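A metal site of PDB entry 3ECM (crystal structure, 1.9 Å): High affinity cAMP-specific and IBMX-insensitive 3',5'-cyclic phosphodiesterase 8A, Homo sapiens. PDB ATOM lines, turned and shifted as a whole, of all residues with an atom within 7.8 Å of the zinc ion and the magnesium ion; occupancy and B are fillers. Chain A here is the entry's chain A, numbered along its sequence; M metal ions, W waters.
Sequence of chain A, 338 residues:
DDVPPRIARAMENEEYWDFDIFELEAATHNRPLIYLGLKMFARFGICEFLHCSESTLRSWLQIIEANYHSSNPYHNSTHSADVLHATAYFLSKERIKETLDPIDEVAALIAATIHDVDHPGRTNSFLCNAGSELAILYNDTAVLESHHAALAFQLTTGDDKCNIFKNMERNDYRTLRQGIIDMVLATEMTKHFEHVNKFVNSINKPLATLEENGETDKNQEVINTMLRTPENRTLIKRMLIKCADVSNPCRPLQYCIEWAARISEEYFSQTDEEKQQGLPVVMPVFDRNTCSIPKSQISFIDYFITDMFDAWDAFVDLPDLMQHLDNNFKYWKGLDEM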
ATOM      1  N   TYR A  68     -14.182  32.656  13.790  1.00  0.00           N
ATOM      2  CA  TYR A  68     -13.282  31.609  13.294  1.00  0.00           C
ATOM      3  C   TYR A  68     -12.912  32.130  11.900  1.00  0.00           C
ATOM      4  O   TYR A  68     -13.792  32.543  11.146  1.00  0.00           O
ATOM      5  CB  TYR A  68     -13.982  30.248  13.161  1.00  0.00           C
ATOM      6  CG  TYR A  68     -13.937  29.403  14.419  1.00  0.00           C
ATOM      7  CD1 TYR A  68     -14.949  29.458  15.374  1.00  0.00           C
ATOM      8  CD2 TYR A  68     -12.847  28.545  14.665  1.00  0.00           C
ATOM      9  CE1 TYR A  68     -14.901  28.673  16.537  1.00  0.00           C
ATOM     10  CE2 TYR A  68     -12.794  27.765  15.834  1.00  0.00           C
ATOM     11  CZ  TYR A  68     -13.827  27.835  16.763  1.00  0.00           C
ATOM     12  OH  TYR A  68     -13.786  27.055  17.898  1.00  0.00           O
ATOM     13  N   TYR A  74      -7.154  25.161   7.621  1.00  0.00           N
ATOM     14  CA  TYR A  74      -7.606  24.172   8.600  1.00  0.00           C
ATOM     15  C   TYR A  74      -8.436  24.730   9.753  1.00  0.00           C
ATOM     16  O   TYR A  74      -9.572  24.322   9.966  1.00  0.00           O
ATOM     17  CB  TYR A  74      -6.408  23.420   9.168  1.00  0.00           C
ATOM     18  CG  TYR A  74      -6.773  22.261  10.075  1.00  0.00           C
ATOM     19  CD1 TYR A  74      -6.929  20.976   9.552  1.00  0.00           C
ATOM     20  CD2 TYR A  74      -6.938  22.435  11.449  1.00  0.00           C
ATOM     21  CE1 TYR A  74      -7.235  19.890  10.372  1.00  0.00           C
ATOM     22  CE2 TYR A  74      -7.238  21.369  12.279  1.00  0.00           C
ATOM     23  CZ  TYR A  74      -7.381  20.093  11.740  1.00  0.00           C
ATOM     24  OH  TYR A  74      -7.665  19.028  12.557  1.00  0.00           O
ATOM     25  N   HIS A  75      -7.840  25.645  10.513  1.00  0.00           N
ATOM     26  CA  HIS A  75      -8.512  26.213  11.679  1.00  0.00           C
ATOM     27  C   HIS A  75      -9.606  27.243  11.399  1.00  0.00           C
ATOM     28  O   HIS A  75      -9.498  28.413  11.785  1.00  0.00           O
ATOM     29  CB  HIS A  75      -7.473  26.796  12.629  1.00  0.00           C
ATOM     30  CG  HIS A  75      -6.632  25.766  13.309  1.00  0.00           C
ATOM     31  ND1 HIS A  75      -5.357  25.451  12.893  1.00  0.00           N
ATOM     32  CD2 HIS A  75      -6.884  24.959  14.365  1.00  0.00           C
ATOM     33  CE1 HIS A  75      -4.854  24.504  13.672  1.00  0.00           C
ATOM     34  NE2 HIS A  75      -5.762  24.190  14.574  1.00  0.00           N
ATOM     35  N   HIS A  79     -13.501  22.989  11.210  1.00  0.00           N
ATOM     36  CA  HIS A  79     -12.729  22.146  12.140  1.00  0.00           C
ATOM     37  C   HIS A  79     -13.451  22.059  13.490  1.00  0.00           C
ATOM     38  O   HIS A  79     -13.574  20.982  14.070  1.00  0.00           O
ATOM     39  CB  HIS A  79     -11.330  22.732  12.361  1.00  0.00           C
ATOM     40  CG  HIS A  79     -10.606  22.135  13.523  1.00  0.00           C
ATOM     41  ND1 HIS A  79     -10.329  20.789  13.625  1.00  0.00           N
ATOM     42  CD2 HIS A  79     -10.098  22.701  14.645  1.00  0.00           C
ATOM     43  CE1 HIS A  79      -9.689  20.547  14.750  1.00  0.00           C
ATOM     44  NE2 HIS A  79      -9.533  21.689  15.389  1.00  0.00           N
ATOM     45  N   SER A  80     -13.949  23.178  13.995  1.00  0.00           N
ATOM     46  CA  SER A  80     -14.642  23.145  15.267  1.00  0.00           C
ATOM     47  C   SER A  80     -15.964  22.394  15.198  1.00  0.00           C
ATOM     48  O   SER A  80     -16.341  21.711  16.154  1.00  0.00           O
ATOM     49  CB  SER A  80     -14.868  24.555  15.797  1.00  0.00           C
ATOM     50  OG  SER A  80     -13.648  25.041  16.330  1.00  0.00           O
ATOM     51  N   VAL A  83     -14.921  18.917  15.471  1.00  0.00           N
ATOM     52  CA  VAL A  83     -14.521  18.552  16.823  1.00  0.00           C
ATOM     53  C   VAL A  83     -15.757  18.456  17.706  1.00  0.00           C
ATOM     54  O   VAL A  83     -15.830  17.619  18.615  1.00  0.00           O
ATOM     55  CB  VAL A  83     -13.517  19.572  17.398  1.00  0.00           C
ATOM     56  CG1 VAL A  83     -13.257  19.293  18.883  1.00  0.00           C
ATOM     57  CG2 VAL A  83     -12.212  19.476  16.621  1.00  0.00           C
ATOM     58  N   ALA A 112     -15.664  22.412  22.890  1.00  0.00           N
ATOM     59  CA  ALA A 112     -15.394  22.017  21.517  1.00  0.00           C
ATOM     60  C   ALA A 112     -15.712  23.168  20.572  1.00  0.00           C
ATOM     61  O   ALA A 112     -14.904  23.542  19.723  1.00  0.00           O
ATOM     62  CB  ALA A 112     -16.233  20.796  21.163  1.00  0.00           C
ATOM     63  N   ILE A 114     -15.900  26.400  21.023  1.00  0.00           N
ATOM     64  CA  ILE A 114     -15.028  27.569  21.116  1.00  0.00           C
ATOM     65  C   ILE A 114     -13.532  27.326  21.191  1.00  0.00           C
ATOM     66  O   ILE A 114     -12.749  28.275  21.070  1.00  0.00           O
ATOM     67  CB  ILE A 114     -15.375  28.403  22.379  1.00  0.00           C
ATOM     68  CG1 ILE A 114     -14.994  27.604  23.625  1.00  0.00           C
ATOM     69  CG2 ILE A 114     -16.876  28.725  22.435  1.00  0.00           C
ATOM     70  CD1 ILE A 114     -15.103  28.385  24.923  1.00  0.00           C
ATOM     71  N   HIS A 115     -13.111  26.078  21.391  1.00  0.00           N
ATOM     72  CA  HIS A 115     -11.696  25.768  21.607  1.00  0.00           C
ATOM     73  C   HIS A 115     -10.620  26.337  20.673  1.00  0.00           C
ATOM     74  O   HIS A 115      -9.448  26.344  21.041  1.00  0.00           O
ATOM     75  CB  HIS A 115     -11.497  24.260  21.734  1.00  0.00           C
ATOM     76  CG  HIS A 115     -11.299  23.580  20.423  1.00  0.00           C
ATOM     77  ND1 HIS A 115     -12.337  23.315  19.552  1.00  0.00           N
ATOM     78  CD2 HIS A 115     -10.172  23.142  19.816  1.00  0.00           C
ATOM     79  CE1 HIS A 115     -11.859  22.755  18.460  1.00  0.00           C
ATOM     80  NE2 HIS A 115     -10.546  22.637  18.593  1.00  0.00           N
ATOM     81  N   ASP A 116     -10.997  26.800  19.491  1.00  0.00           N
ATOM     82  CA  ASP A 116     -10.015  27.370  18.564  1.00  0.00           C
ATOM     83  C   ASP A 116     -10.442  28.726  18.002  1.00  0.00           C
ATOM     84  O   ASP A 116      -9.880  29.176  16.986  1.00  0.00           O
ATOM     85  CB  ASP A 116      -9.787  26.426  17.388  1.00  0.00           C
ATOM     86  CG  ASP A 116      -8.656  25.458  17.620  1.00  0.00           C
ATOM     87  OD1 ASP A 116      -7.782  25.769  18.453  1.00  0.00           O
ATOM     88  OD2 ASP A 116      -8.623  24.402  16.954  1.00  0.00           O
ATOM     89  N   VAL A 117     -11.402  29.380  18.639  1.00  0.00           N
ATOM     90  CA  VAL A 117     -11.909  30.659  18.152  1.00  0.00           C
ATOM     91  C   VAL A 117     -10.838  31.723  17.938  1.00  0.00           C
ATOM     92  O   VAL A 117      -9.955  31.926  18.764  1.00  0.00           O
ATOM     93  CB  VAL A 117     -13.027  31.221  19.080  1.00  0.00           C
ATOM     94  CG1 VAL A 117     -12.427  31.761  20.378  1.00  0.00           C
ATOM     95  CG2 VAL A 117     -13.819  32.308  18.333  1.00  0.00           C
ATOM     96  N   HIS A 119      -8.419  31.632  15.923  1.00  0.00           N
ATOM     97  CA  HIS A 119      -7.097  31.044  15.681  1.00  0.00           C
ATOM     98  C   HIS A 119      -6.568  31.763  14.425  1.00  0.00           C
ATOM     99  O   HIS A 119      -7.304  31.953  13.456  1.00  0.00           O
ATOM    100  CB  HIS A 119      -7.268  29.542  15.418  1.00  0.00           C
ATOM    101  CG  HIS A 119      -5.991  28.767  15.449  1.00  0.00           C
ATOM    102  ND1 HIS A 119      -4.946  29.010  14.581  1.00  0.00           N
ATOM    103  CD2 HIS A 119      -5.587  27.741  16.244  1.00  0.00           C
ATOM    104  CE1 HIS A 119      -3.961  28.176  14.837  1.00  0.00           C
ATOM    105  NE2 HIS A 119      -4.327  27.390  15.839  1.00  0.00           N
ATOM    106  N   ASN A 124       1.764  28.433  18.297  1.00  0.00           N
ATOM    107  CA  ASN A 124       2.181  29.275  19.421  1.00  0.00           C
ATOM    108  C   ASN A 124       3.628  29.712  19.228  1.00  0.00           C
ATOM    109  O   ASN A 124       3.977  30.870  19.452  1.00  0.00           O
ATOM    110  CB  ASN A 124       2.061  28.527  20.762  1.00  0.00           C
ATOM    111  CG  ASN A 124       0.621  28.414  21.245  1.00  0.00           C
ATOM    112  OD1 ASN A 124      -0.155  29.362  21.159  1.00  0.00           O
ATOM    113  ND2 ASN A 124       0.267  27.254  21.777  1.00  0.00           N
ATOM    114  N   LEU A 144      -2.220  30.704  22.290  1.00  0.00           N
ATOM    115  CA  LEU A 144      -3.497  30.586  21.587  1.00  0.00           C
ATOM    116  C   LEU A 144      -4.644  30.034  22.425  1.00  0.00           C
ATOM    117  O   LEU A 144      -5.764  30.545  22.365  1.00  0.00           O
ATOM    118  CB  LEU A 144      -3.335  29.753  20.308  1.00  0.00           C
ATOM    119  CG  LEU A 144      -2.638  30.481  19.147  1.00  0.00           C
ATOM    120  CD1 LEU A 144      -2.715  29.625  17.895  1.00  0.00           C
ATOM    121  CD2 LEU A 144      -3.313  31.821  18.906  1.00  0.00           C
ATOM    122  N   GLU A 145      -4.356  28.996  23.196  1.00  0.00           N
ATOM    123  CA  GLU A 145      -5.395  28.376  24.027  1.00  0.00           C
ATOM    124  C   GLU A 145      -5.970  29.379  25.034  1.00  0.00           C
ATOM    125  O   GLU A 145      -7.181  29.400  25.276  1.00  0.00           O
ATOM    126  CB  GLU A 145      -4.848  27.144  24.757  1.00  0.00           C
ATOM    127  CG  GLU A 145      -4.520  25.945  23.864  1.00  0.00           C
ATOM    128  CD  GLU A 145      -3.293  26.163  22.990  1.00  0.00           C
ATOM    129  OE1 GLU A 145      -2.437  26.993  23.340  1.00  0.00           O
ATOM    130  OE2 GLU A 145      -3.176  25.464  21.958  1.00  0.00           O
ATOM    131  N   HIS A 148      -8.191  31.660  23.024  1.00  0.00           N
ATOM    132  CA  HIS A 148      -9.465  31.067  22.602  1.00  0.00           C
ATOM    133  C   HIS A 148     -10.480  31.134  23.741  1.00  0.00           C
ATOM    134  O   HIS A 148     -11.630  31.541  23.551  1.00  0.00           O
ATOM    135  CB  HIS A 148      -9.291  29.599  22.185  1.00  0.00           C
ATOM    136  CG  HIS A 148      -8.306  29.384  21.084  1.00  0.00           C
ATOM    137  ND1 HIS A 148      -8.256  30.168  19.955  1.00  0.00           N
ATOM    138  CD2 HIS A 148      -7.321  28.455  20.932  1.00  0.00           C
ATOM    139  CE1 HIS A 148      -7.288  29.749  19.165  1.00  0.00           C
ATOM    140  NE2 HIS A 148      -6.706  28.709  19.729  1.00  0.00           N
ATOM    141  N   VAL A 184     -10.389  23.705  27.344  1.00  0.00           N
ATOM    142  CA  VAL A 184      -9.758  24.481  26.279  1.00  0.00           C
ATOM    143  C   VAL A 184      -8.243  24.528  26.457  1.00  0.00           C
ATOM    144  O   VAL A 184      -7.495  24.372  25.492  1.00  0.00           O
ATOM    145  CB  VAL A 184     -10.312  25.920  26.225  1.00  0.00           C
ATOM    146  CG1 VAL A 184      -9.533  26.736  25.213  1.00  0.00           C
ATOM    147  CG2 VAL A 184     -11.795  25.884  25.837  1.00  0.00           C
ATOM    148  N   THR A 187      -6.008  21.523  25.409  1.00  0.00           N
ATOM    149  CA  THR A 187      -5.743  21.251  24.000  1.00  0.00           C
ATOM    150  C   THR A 187      -4.356  21.723  23.556  1.00  0.00           C
ATOM    151  O   THR A 187      -3.960  21.499  22.412  1.00  0.00           O
ATOM    152  CB  THR A 187      -6.779  21.905  23.073  1.00  0.00           C
ATOM    153  OG1 THR A 187      -6.743  23.323  23.234  1.00  0.00           O
ATOM    154  CG2 THR A 187      -8.167  21.384  23.379  1.00  0.00           C
ATOM    155  N   GLU A 188      -3.628  22.409  24.439  1.00  0.00           N
ATOM    156  CA  GLU A 188      -2.282  22.854  24.091  1.00  0.00           C
ATOM    157  C   GLU A 188      -1.401  21.610  23.989  1.00  0.00           C
ATOM    158  O   GLU A 188      -1.255  20.861  24.964  1.00  0.00           O
ATOM    159  CB  GLU A 188      -1.728  23.799  25.166  1.00  0.00           C
ATOM    160  CG  GLU A 188      -0.269  24.161  24.937  1.00  0.00           C
ATOM    161  CD  GLU A 188       0.271  25.106  25.978  1.00  0.00           C
ATOM    162  OE1 GLU A 188      -0.072  24.942  27.166  1.00  0.00           O
ATOM    163  OE2 GLU A 188       1.058  25.997  25.607  1.00  0.00           O
ATOM    164  N   MET A 189      -0.804  21.391  22.814  1.00  0.00           N
ATOM    165  CA  MET A 189       0.000  20.181  22.608  1.00  0.00           C
ATOM    166  C   MET A 189       1.266  19.956  23.420  1.00  0.00           C
ATOM    167  O   MET A 189       1.648  18.809  23.638  1.00  0.00           O
ATOM    168  CB  MET A 189       0.312  20.026  21.113  1.00  0.00           C
ATOM    169  CG  MET A 189      -0.906  19.597  20.297  1.00  0.00           C
ATOM    170  SD  MET A 189      -1.775  18.171  21.014  1.00  0.00           S
ATOM    171  CE  MET A 189      -0.803  16.833  20.321  1.00  0.00           C
ATOM    172  N   ILE A 241     -11.707  15.817  25.079  1.00  0.00           N
ATOM    173  CA  ILE A 241     -11.538  16.946  24.174  1.00  0.00           C
ATOM    174  C   ILE A 241     -10.251  16.809  23.355  1.00  0.00           C
ATOM    175  O   ILE A 241     -10.213  17.191  22.179  1.00  0.00           O
ATOM    176  CB  ILE A 241     -11.520  18.310  24.952  1.00  0.00           C
ATOM    177  CG1 ILE A 241     -11.571  19.476  23.967  1.00  0.00           C
ATOM    178  CG2 ILE A 241     -10.276  18.425  25.813  1.00  0.00           C
ATOM    179  CD1 ILE A 241     -12.853  19.539  23.179  1.00  0.00           C
ATOM    180  N   ALA A 244     -10.958  14.317  20.613  1.00  0.00           N
ATOM    181  CA  ALA A 244     -11.876  14.871  19.609  1.00  0.00           C
ATOM    182  C   ALA A 244     -11.109  15.854  18.721  1.00  0.00           C
ATOM    183  O   ALA A 244     -11.298  15.876  17.513  1.00  0.00           O
ATOM    184  CB  ALA A 244     -13.048  15.577  20.282  1.00  0.00           C
ATOM    185  N   ASP A 245     -10.230  16.642  19.339  1.00  0.00           N
ATOM    186  CA  ASP A 245      -9.435  17.654  18.643  1.00  0.00           C
ATOM    187  C   ASP A 245      -8.533  17.063  17.554  1.00  0.00           C
ATOM    188  O   ASP A 245      -8.346  17.681  16.506  1.00  0.00           O
ATOM    189  CB  ASP A 245      -8.596  18.433  19.664  1.00  0.00           C
ATOM    190  CG  ASP A 245      -8.061  19.765  19.114  1.00  0.00           C
ATOM    191  OD1 ASP A 245      -8.460  20.196  18.003  1.00  0.00           O
ATOM    192  OD2 ASP A 245      -7.251  20.415  19.820  1.00  0.00           O
ATOM    193  N   VAL A 246      -7.966  15.880  17.787  1.00  0.00           N
ATOM    194  CA  VAL A 246      -7.083  15.283  16.791  1.00  0.00           C
ATOM    195  C   VAL A 246      -7.604  13.946  16.290  1.00  0.00           C
ATOM    196  O   VAL A 246      -6.852  12.989  16.105  1.00  0.00           O
ATOM    197  CB  VAL A 246      -5.648  15.121  17.343  1.00  0.00           C
ATOM    198  CG1 VAL A 246      -5.118  16.481  17.789  1.00  0.00           C
ATOM    199  CG2 VAL A 246      -5.630  14.155  18.528  1.00  0.00           C
HETATM  200 ZN    ZN M   1      -8.580  22.255  17.357  1.00  0.00          ZN
HETATM  201 MG    MG M   2      -6.070  24.691  19.377  1.00  0.00          MG
HETATM  202  O   HOH W   1      -6.783  22.573  18.794  1.00  0.00           O
HETATM  203  O   HOH W   2      -5.037  26.670  19.359  1.00  0.00           O
HETATM  204  O   HOH W   3      -7.424  24.913  21.278  1.00  0.00           O
HETATM  205  O   HOH W   4      -6.454  21.883  16.220  1.00  0.00           O
HETATM  206  O   HOH W   5      -5.056  23.843  17.415  1.00  0.00           O
HETATM  207  O   HOH W   6      -4.444  23.753  20.542  1.00  0.00           O
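N of Asp 116 sits at hydrogen-bond distance from OH of Tyr 68 (3.2 Å). The side-chain carboxylate of Asp 116 lies close to a ring nitrogen (NE2) of His 148, at 3.4 Å. A ring nitrogen (ND1) of His 115 lies within hydrogen-bond range of the backbone carbonyl oxygen (O) of Ala 112, 2.6 Å away. ND1 of His 79 lies close to OH of Tyr 74 (3.4 Å). OE1 of Glu 145 lies within hydrogen-bond range of ND2 of Asn 124 (3.1 Å).
Within 4 Å of the zinc ion: His 79, His 115, Asp 116 and Asp 245. The nearest printed residue that does not touch the zinc ion is His 75 (4.4 Å).
OE2 of Glu 145 touches the magnesium ion, at 3.95 Å. Of the 24 residues printed, 2 come within 4 Å of the magnesium ion. Along chain A the residues within 4 Å of the magnesium ion span positions 116 to 145. The nearest printed residue that does not touch the magnesium ion is His 148 (4.1 Å).
The zinc ion is bound by OD1 of Asp 245 (2.2 Å), OD2 of Asp 116 (2.2 Å), NE2 of His 79 (2.3 Å), water W1 (2.3 Å), NE2 of His 115 (2.4 Å) and water W4 (2.4 Å).
Water W6 is bound to the magnesium ion, 2.2 Å away. OD1 of Asp 116 binds the magnesium ion (2.2 Å). Water W2 binds the magnesium ion (2.2 Å). Water W1 binds the magnesium ion (2.3 Å). Water W3 is bound to the magnesium ion (2.3 Å). Water W5 binds the magnesium ion. The magnesium ion has six donor atoms within binding distance.
Water W2 lies within hydrogen-bond range of a ring nitrogen (NE2) of His 148 and the side-chain carboxylate (OE2) of Glu 145. Water W6 bridges OE2 of Glu 145 (2.6 Å) and O of Thr 187 (3.0 Å). Water W3 lies within hydrogen-bond range of the backbone carbonyl oxygen of His 115 and the side-chain hydroxyl of Thr 187.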
